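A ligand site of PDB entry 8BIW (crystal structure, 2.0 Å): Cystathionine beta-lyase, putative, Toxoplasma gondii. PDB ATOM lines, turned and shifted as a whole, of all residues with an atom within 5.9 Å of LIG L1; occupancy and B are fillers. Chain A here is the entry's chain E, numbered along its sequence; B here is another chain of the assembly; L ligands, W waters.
Merely in contact with LIG L1: Thr 107, Tyr 133, Asn 180, Thr 207, Phe 208, Gly 240 and Leu 361. Of the 24 residues printed, 15 come within 4 Å of LIG L1.
The backbone carbonyl oxygen (O) of Gly 240 is in hydrogen-bond range of the backbone NH (N) of Thr 228. N of Asn 180 lies within hydrogen-bond range of OE1 of Glu 176 (2.8 Å). The backbone NH (N) of Tyr 133 is in hydrogen-bond range of the side-chain carboxylate (OE2) of Glu 176 (3.0 Å). The side-chain hydroxyl (OG1) of Thr 107 is in hydrogen-bond range of the backbone NH (N) of Ala 110 (3.0 Å). The side-chain hydroxyl of Thr 229 is in hydrogen-bond range of the backbone NH of Gly 240, at 3.0 Å. The side-chain hydroxyl of Thr 107 is in hydrogen-bond range of the backbone carbonyl oxygen of Gly 262 of chain B (2.7 Å). N of Ser 227 is in hydrogen-bond range of OG1 of Thr 207. N of Met 109 sits close to OG1 of Thr 107.
The backbone NH (N) of Gly 108 sits at hydrogen-bond distance from an oxygen (O5) of LIG L1, at 2.9 Å. The guanidinium group (NE) of Arg 80 of chain B lies within salt-bridge range of an oxygen (O3) of LIG L1. The side-chain hydroxyl (OG1) of Thr 229 sits at hydrogen-bond distance from an oxygen (O5) of LIG L1 (2.7 Å). The side-chain hydroxyl (OH) of Tyr 133 is covalently linked to a carbon (C3) of LG2 L2 (1.4 Å). The backbone NH of Met 109 lies within hydrogen-bond range of an oxygen (O3) of LIG L1, 2.8 Å away. O4 of LIG L1 lies within hydrogen-bond range of OH of Tyr 78 of chain B (2.5 Å). O5 of LIG L1 lies within hydrogen-bond range of OG of Ser 227 (2.7 Å). NZ of Lys 230 is bonded to C5 of LIG L1, 1.4 Å away. The side-chain carboxylate (OD2) of Asp 205 is in hydrogen-bond range of a nitrogen (N1) of LIG L1, at 2.6 Å. A nitrogen (N1) of LG2 L2 sits close to the side-chain amino group of Lys 230 (3.1 Å).
Water W1 lies within hydrogen-bond range of the side-chain hydroxyl (OG1) of Thr 136, the side-chain hydroxyl (OG1) of Thr 112 and the side-chain sulfur (SD) of Met 109.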
ATOM      1  N   THR A 107     -31.884  -8.959 -18.206  1.00  0.00           N
ATOM      2  CA  THR A 107     -31.533  -9.458 -16.885  1.00  0.00           C
ATOM      3  C   THR A 107     -30.151 -10.114 -16.919  1.00  0.00           C
ATOM      4  O   THR A 107     -29.625 -10.454 -17.980  1.00  0.00           O
ATOM      5  CB  THR A 107     -32.525 -10.550 -16.344  1.00  0.00           C
ATOM      6  OG1 THR A 107     -32.456 -11.698 -17.207  1.00  0.00           O
ATOM      7  CG2 THR A 107     -34.028 -10.083 -16.216  1.00  0.00           C
ATOM      8  N   GLY A 108     -29.600 -10.385 -15.732  1.00  0.00           N
ATOM      9  CA  GLY A 108     -28.359 -11.165 -15.655  1.00  0.00           C
ATOM     10  C   GLY A 108     -28.553 -12.594 -16.158  1.00  0.00           C
ATOM     11  O   GLY A 108     -27.651 -13.168 -16.774  1.00  0.00           O
ATOM     12  N   MET A 109     -29.734 -13.190 -15.902  1.00  0.00           N
ATOM     13  CA  MET A 109     -29.969 -14.548 -16.398  1.00  0.00           C
ATOM     14  C   MET A 109     -29.963 -14.559 -17.919  1.00  0.00           C
ATOM     15  O   MET A 109     -29.460 -15.487 -18.551  1.00  0.00           O
ATOM     16  CB  MET A 109     -31.288 -15.111 -15.885  1.00  0.00           C
ATOM     17  CG  MET A 109     -31.287 -15.758 -14.513  1.00  0.00           C
ATOM     18  SD  MET A 109     -29.842 -16.802 -14.219  1.00  0.00           S
ATOM     19  CE  MET A 109     -29.981 -18.045 -15.511  1.00  0.00           C
ATOM     20  N   ALA A 110     -30.546 -13.517 -18.532  1.00  0.00           N
ATOM     21  CA  ALA A 110     -30.498 -13.427 -20.008  1.00  0.00           C
ATOM     22  C   ALA A 110     -29.074 -13.332 -20.517  1.00  0.00           C
ATOM     23  O   ALA A 110     -28.737 -13.917 -21.567  1.00  0.00           O
ATOM     24  CB  ALA A 110     -31.255 -12.203 -20.515  1.00  0.00           C
ATOM     25  N   THR A 112     -26.410 -14.604 -19.095  1.00  0.00           N
ATOM     26  CA  THR A 112     -25.801 -15.918 -18.885  1.00  0.00           C
ATOM     27  C   THR A 112     -26.274 -16.924 -19.917  1.00  0.00           C
ATOM     28  O   THR A 112     -25.482 -17.701 -20.494  1.00  0.00           O
ATOM     29  CB  THR A 112     -26.173 -16.410 -17.478  1.00  0.00           C
ATOM     30  OG1 THR A 112     -25.659 -15.467 -16.518  1.00  0.00           O
ATOM     31  CG2 THR A 112     -25.665 -17.823 -17.194  1.00  0.00           C
ATOM     32  N   TYR A 133     -24.489 -19.205  -8.553  1.00  0.00           N
ATOM     33  CA  TYR A 133     -25.833 -18.661  -8.345  1.00  0.00           C
ATOM     34  C   TYR A 133     -26.847 -19.719  -8.776  1.00  0.00           C
ATOM     35  O   TYR A 133     -26.695 -20.341  -9.849  1.00  0.00           O
ATOM     36  CB  TYR A 133     -26.019 -17.362  -9.145  1.00  0.00           C
ATOM     37  CG  TYR A 133     -27.440 -16.865  -9.104  1.00  0.00           C
ATOM     38  CD1 TYR A 133     -28.203 -16.689 -10.257  1.00  0.00           C
ATOM     39  CD2 TYR A 133     -28.032 -16.601  -7.889  1.00  0.00           C
ATOM     40  CE1 TYR A 133     -29.535 -16.218 -10.162  1.00  0.00           C
ATOM     41  CE2 TYR A 133     -29.315 -16.160  -7.786  1.00  0.00           C
ATOM     42  CZ  TYR A 133     -30.075 -15.962  -8.898  1.00  0.00           C
ATOM     43  OH  TYR A 133     -31.373 -15.495  -8.670  1.00  0.00           O
ATOM     44  N   THR A 136     -28.261 -19.966 -12.408  1.00  0.00           N
ATOM     45  CA  THR A 136     -27.312 -20.476 -13.390  1.00  0.00           C
ATOM     46  C   THR A 136     -27.351 -22.005 -13.420  1.00  0.00           C
ATOM     47  O   THR A 136     -27.444 -22.636 -14.493  1.00  0.00           O
ATOM     48  CB  THR A 136     -25.910 -19.985 -13.030  1.00  0.00           C
ATOM     49  OG1 THR A 136     -25.956 -18.552 -12.883  1.00  0.00           O
ATOM     50  CG2 THR A 136     -24.848 -20.409 -14.098  1.00  0.00           C
ATOM     51  N   GLU A 176     -17.274 -18.066 -11.012  1.00  0.00           N
ATOM     52  CA  GLU A 176     -17.991 -17.019 -10.326  1.00  0.00           C
ATOM     53  C   GLU A 176     -17.150 -16.643  -9.127  1.00  0.00           C
ATOM     54  O   GLU A 176     -16.744 -17.530  -8.386  1.00  0.00           O
ATOM     55  CB  GLU A 176     -19.362 -17.539  -9.913  1.00  0.00           C
ATOM     56  CG  GLU A 176     -20.290 -16.593  -9.210  1.00  0.00           C
ATOM     57  CD  GLU A 176     -21.666 -17.224  -8.997  1.00  0.00           C
ATOM     58  OE1 GLU A 176     -22.018 -17.410  -7.833  1.00  0.00           O
ATOM     59  OE2 GLU A 176     -22.391 -17.542  -9.982  1.00  0.00           O
ATOM     60  N   PRO A 178     -16.628 -13.506  -5.893  1.00  0.00           N
ATOM     61  CA  PRO A 178     -16.986 -14.499  -4.872  1.00  0.00           C
ATOM     62  C   PRO A 178     -18.235 -15.274  -5.313  1.00  0.00           C
ATOM     63  O   PRO A 178     -19.013 -14.716  -6.092  1.00  0.00           O
ATOM     64  CB  PRO A 178     -17.308 -13.649  -3.612  1.00  0.00           C
ATOM     65  CG  PRO A 178     -16.556 -12.337  -3.830  1.00  0.00           C
ATOM     66  CD  PRO A 178     -16.648 -12.128  -5.360  1.00  0.00           C
ATOM     67  N   ASN A 180     -21.881 -17.115  -5.075  1.00  0.00           N
ATOM     68  CA  ASN A 180     -23.183 -17.042  -4.422  1.00  0.00           C
ATOM     69  C   ASN A 180     -23.559 -18.405  -3.863  1.00  0.00           C
ATOM     70  O   ASN A 180     -23.653 -19.362  -4.635  1.00  0.00           O
ATOM     71  CB  ASN A 180     -24.217 -16.622  -5.456  1.00  0.00           C
ATOM     72  CG  ASN A 180     -25.497 -16.148  -4.841  1.00  0.00           C
ATOM     73  OD1 ASN A 180     -25.759 -16.346  -3.641  1.00  0.00           O
ATOM     74  ND2 ASN A 180     -26.312 -15.460  -5.658  1.00  0.00           N
ATOM     75  N   ASP A 205     -18.423 -14.830 -13.909  1.00  0.00           N
ATOM     76  CA  ASP A 205     -19.519 -14.045 -13.311  1.00  0.00           C
ATOM     77  C   ASP A 205     -18.974 -13.312 -12.073  1.00  0.00           C
ATOM     78  O   ASP A 205     -18.865 -13.878 -10.971  1.00  0.00           O
ATOM     79  CB  ASP A 205     -20.695 -14.935 -12.938  1.00  0.00           C
ATOM     80  CG  ASP A 205     -21.903 -14.157 -12.376  1.00  0.00           C
ATOM     81  OD1 ASP A 205     -21.794 -12.981 -11.938  1.00  0.00           O
ATOM     82  OD2 ASP A 205     -22.994 -14.736 -12.343  1.00  0.00           O
ATOM     83  N   THR A 207     -20.391 -10.669 -10.567  1.00  0.00           N
ATOM     84  CA  THR A 207     -21.457  -9.860  -9.976  1.00  0.00           C
ATOM     85  C   THR A 207     -21.184  -9.494  -8.514  1.00  0.00           C
ATOM     86  O   THR A 207     -21.369  -8.330  -8.128  1.00  0.00           O
ATOM     87  CB  THR A 207     -22.797 -10.604 -10.058  1.00  0.00           C
ATOM     88  OG1 THR A 207     -23.203 -10.800 -11.432  1.00  0.00           O
ATOM     89  CG2 THR A 207     -23.905  -9.835  -9.301  1.00  0.00           C
ATOM     90  N   PHE A 208     -20.770 -10.420  -7.665  1.00  0.00           N
ATOM     91  CA  PHE A 208     -20.565 -10.122  -6.238  1.00  0.00           C
ATOM     92  C   PHE A 208     -19.394  -9.192  -5.977  1.00  0.00           C
ATOM     93  O   PHE A 208     -19.327  -8.531  -5.003  1.00  0.00           O
ATOM     94  CB  PHE A 208     -20.382 -11.396  -5.453  1.00  0.00           C
ATOM     95  CG  PHE A 208     -21.637 -12.061  -5.003  1.00  0.00           C
ATOM     96  CD1 PHE A 208     -22.801 -11.981  -5.733  1.00  0.00           C
ATOM     97  CD2 PHE A 208     -21.642 -12.815  -3.844  1.00  0.00           C
ATOM     98  CE1 PHE A 208     -23.940 -12.618  -5.317  1.00  0.00           C
ATOM     99  CE2 PHE A 208     -22.774 -13.451  -3.422  1.00  0.00           C
ATOM    100  CZ  PHE A 208     -23.928 -13.357  -4.151  1.00  0.00           C
ATOM    101  N   SER A 227     -24.801  -9.469 -13.492  1.00  0.00           N
ATOM    102  CA  SER A 227     -26.163  -9.027 -13.216  1.00  0.00           C
ATOM    103  C   SER A 227     -26.054  -7.554 -12.821  1.00  0.00           C
ATOM    104  O   SER A 227     -25.606  -7.237 -11.705  1.00  0.00           O
ATOM    105  CB  SER A 227     -26.774  -9.824 -12.075  1.00  0.00           C
ATOM    106  OG  SER A 227     -28.070  -9.310 -11.778  1.00  0.00           O
ATOM    107  N   THR A 228     -26.450  -6.647 -13.735  1.00  0.00           N
ATOM    108  CA  THR A 228     -26.390  -5.234 -13.383  1.00  0.00           C
ATOM    109  C   THR A 228     -27.497  -4.869 -12.394  1.00  0.00           C
ATOM    110  O   THR A 228     -27.407  -3.803 -11.743  1.00  0.00           O
ATOM    111  CB  THR A 228     -26.465  -4.346 -14.652  1.00  0.00           C
ATOM    112  OG1 THR A 228     -27.767  -4.460 -15.251  1.00  0.00           O
ATOM    113  CG2 THR A 228     -25.452  -4.790 -15.673  1.00  0.00           C
ATOM    114  N   THR A 229     -28.488  -5.752 -12.246  1.00  0.00           N
ATOM    115  CA  THR A 229     -29.509  -5.664 -11.179  1.00  0.00           C
ATOM    116  C   THR A 229     -28.899  -5.348  -9.818  1.00  0.00           C
ATOM    117  O   THR A 229     -29.532  -4.684  -8.990  1.00  0.00           O
ATOM    118  CB  THR A 229     -30.254  -7.018 -11.074  1.00  0.00           C
ATOM    119  OG1 THR A 229     -30.699  -7.437 -12.367  1.00  0.00           O
ATOM    120  CG2 THR A 229     -31.405  -6.978 -10.078  1.00  0.00           C
ATOM    121  N   LYS A 230     -27.755  -5.950  -9.524  1.00  0.00           N
ATOM    122  CA  LYS A 230     -27.290  -6.011  -8.137  1.00  0.00           C
ATOM    123  C   LYS A 230     -26.540  -4.738  -7.748  1.00  0.00           C
ATOM    124  O   LYS A 230     -27.145  -3.802  -7.230  1.00  0.00           O
ATOM    125  CB  LYS A 230     -26.383  -7.257  -7.951  1.00  0.00           C
ATOM    126  CG  LYS A 230     -27.036  -8.590  -8.354  1.00  0.00           C
ATOM    127  CD  LYS A 230     -28.427  -8.654  -7.952  1.00  0.00           C
ATOM    128  CE  LYS A 230     -29.000 -10.123  -7.848  1.00  0.00           C
ATOM    129  NZ  LYS A 230     -28.446 -11.179  -8.745  1.00  0.00           N
ATOM    130  N   LEU A 239     -33.886  -4.399 -13.317  1.00  0.00           N
ATOM    131  CA  LEU A 239     -33.228  -5.658 -13.711  1.00  0.00           C
ATOM    132  C   LEU A 239     -32.299  -5.377 -14.879  1.00  0.00           C
ATOM    133  O   LEU A 239     -32.580  -4.540 -15.717  1.00  0.00           O
ATOM    134  CB  LEU A 239     -34.277  -6.688 -14.167  1.00  0.00           C
ATOM    135  CG  LEU A 239     -35.363  -7.092 -13.186  1.00  0.00           C
ATOM    136  CD1 LEU A 239     -36.427  -7.981 -13.850  1.00  0.00           C
ATOM    137  CD2 LEU A 239     -34.701  -7.827 -12.003  1.00  0.00           C
ATOM    138  N   GLY A 240     -31.214  -6.119 -14.981  1.00  0.00           N
ATOM    139  CA  GLY A 240     -30.368  -5.925 -16.177  1.00  0.00           C
ATOM    140  C   GLY A 240     -29.215  -6.902 -16.138  1.00  0.00           C
ATOM    141  O   GLY A 240     -28.896  -7.475 -15.100  1.00  0.00           O
ATOM    142  N   GLY A 241     -28.636  -7.126 -17.313  1.00  0.00           N
ATOM    143  CA  GLY A 241     -27.454  -7.928 -17.429  1.00  0.00           C
ATOM    144  C   GLY A 241     -26.477  -7.311 -18.404  1.00  0.00           C
ATOM    145  O   GLY A 241     -26.835  -6.474 -19.260  1.00  0.00           O
ATOM    146  N   LEU A 361     -29.573  -8.509  -3.759  1.00  0.00           N
ATOM    147  CA  LEU A 361     -28.357  -8.140  -3.045  1.00  0.00           C
ATOM    148  C   LEU A 361     -27.786  -6.929  -3.757  1.00  0.00           C
ATOM    149  O   LEU A 361     -28.196  -6.615  -4.883  1.00  0.00           O
ATOM    150  CB  LEU A 361     -27.330  -9.295  -3.034  1.00  0.00           C
ATOM    151  CG  LEU A 361     -26.974  -9.816  -4.446  1.00  0.00           C
ATOM    152  CD1 LEU A 361     -25.624  -9.336  -4.938  1.00  0.00           C
ATOM    153  CD2 LEU A 361     -27.068 -11.362  -4.485  1.00  0.00           C
ATOM    154  N   TYR B  78     -39.516 -11.601  -6.753  1.00  0.00           N
ATOM    155  CA  TYR B  78     -38.424 -11.036  -7.559  1.00  0.00           C
ATOM    156  C   TYR B  78     -38.934 -10.754  -8.970  1.00  0.00           C
ATOM    157  O   TYR B  78     -39.599 -11.602  -9.555  1.00  0.00           O
ATOM    158  CB  TYR B  78     -37.281 -12.045  -7.613  1.00  0.00           C
ATOM    159  CG  TYR B  78     -35.994 -11.527  -8.160  1.00  0.00           C
ATOM    160  CD1 TYR B  78     -35.279 -10.552  -7.496  1.00  0.00           C
ATOM    161  CD2 TYR B  78     -35.468 -12.054  -9.337  1.00  0.00           C
ATOM    162  CE1 TYR B  78     -34.048 -10.116  -7.979  1.00  0.00           C
ATOM    163  CE2 TYR B  78     -34.267 -11.606  -9.864  1.00  0.00           C
ATOM    164  CZ  TYR B  78     -33.570 -10.621  -9.180  1.00  0.00           C
ATOM    165  OH  TYR B  78     -32.356 -10.158  -9.662  1.00  0.00           O
ATOM    166  N   ARG B  80     -37.721 -10.620 -11.960  1.00  0.00           N
ATOM    167  CA  ARG B  80     -37.418 -11.460 -13.121  1.00  0.00           C
ATOM    168  C   ARG B  80     -38.465 -12.577 -13.266  1.00  0.00           C
ATOM    169  O   ARG B  80     -38.792 -13.014 -14.384  1.00  0.00           O
ATOM    170  CB  ARG B  80     -36.001 -12.056 -13.015  1.00  0.00           C
ATOM    171  CG  ARG B  80     -35.805 -13.217 -14.062  1.00  0.00           C
ATOM    172  CD  ARG B  80     -34.329 -13.625 -14.356  1.00  0.00           C
ATOM    173  NE  ARG B  80     -33.467 -13.613 -13.161  1.00  0.00           N
ATOM    174  CZ  ARG B  80     -33.516 -14.458 -12.126  1.00  0.00           C
ATOM    175  NH1 ARG B  80     -34.435 -15.407 -12.042  1.00  0.00           N
ATOM    176  NH2 ARG B  80     -32.625 -14.321 -11.143  1.00  0.00           N
ATOM    177  N   GLY B 262     -34.639 -15.301 -18.314  1.00  0.00           N
ATOM    178  CA  GLY B 262     -34.458 -13.920 -17.929  1.00  0.00           C
ATOM    179  C   GLY B 262     -34.976 -12.929 -18.944  1.00  0.00           C
ATOM    180  O   GLY B 262     -34.421 -11.839 -19.050  1.00  0.00           O
HETATM  181  N1  LIG L   1     -25.277 -14.230 -11.101  1.00  0.00           N
HETATM  182  C1  LIG L   1     -25.254 -13.776  -9.837  1.00  0.00           C
HETATM  183  C2  LIG L   1     -23.951 -13.929  -9.027  1.00  0.00           C
HETATM  184  C3  LIG L   1     -26.211 -13.277  -9.413  1.00  0.00           C
HETATM  185  O1  LIG L   1     -26.177 -12.764  -8.108  1.00  0.00           O
HETATM  186  C4  LIG L   1     -27.493 -13.109 -10.172  1.00  0.00           C
HETATM  187  C5  LIG L   1     -28.636 -12.427  -9.421  1.00  0.00           C
HETATM  188  C6  LIG L   1     -27.628 -13.509 -11.260  1.00  0.00           C
HETATM  189  C7  LIG L   1     -26.538 -14.107 -11.909  1.00  0.00           C
HETATM  190  C8  LIG L   1     -28.930 -13.404 -12.095  1.00  0.00           C
HETATM  191  O2  LIG L   1     -29.080 -12.057 -12.472  1.00  0.00           O
HETATM  192  P1  LIG L   1     -30.645 -11.500 -12.629  1.00  0.00           P
HETATM  193  O3  LIG L   1     -31.282 -12.306 -13.759  1.00  0.00           O
HETATM  194  O4  LIG L   1     -31.306 -11.757 -11.286  1.00  0.00           O
HETATM  195  O5  LIG L   1     -30.413 -10.028 -12.936  1.00  0.00           O
HETATM  196  C1  LG2 L   2     -33.878 -16.046  -8.394  1.00  0.00           C
HETATM  197  C2  LG2 L   2     -33.351 -15.229  -7.479  1.00  0.00           C
HETATM  198  C3  LG2 L   2     -31.867 -14.825  -7.570  1.00  0.00           C
HETATM  199  C4  LG2 L   2     -31.606 -13.619  -6.657  1.00  0.00           C
HETATM  200  C5  LG2 L   2     -30.900 -13.995  -5.328  1.00  0.00           C
HETATM  201  O1  LG2 L   2     -29.710 -14.486  -5.295  1.00  0.00           O
HETATM  202  O2  LG2 L   2     -31.552 -13.796  -4.235  1.00  0.00           O
HETATM  203  N1  LG2 L   2     -30.805 -12.662  -7.389  1.00  0.00           N
HETATM  204  O   HOH W   1     -26.596 -16.218 -13.915  1.00  0.00           O
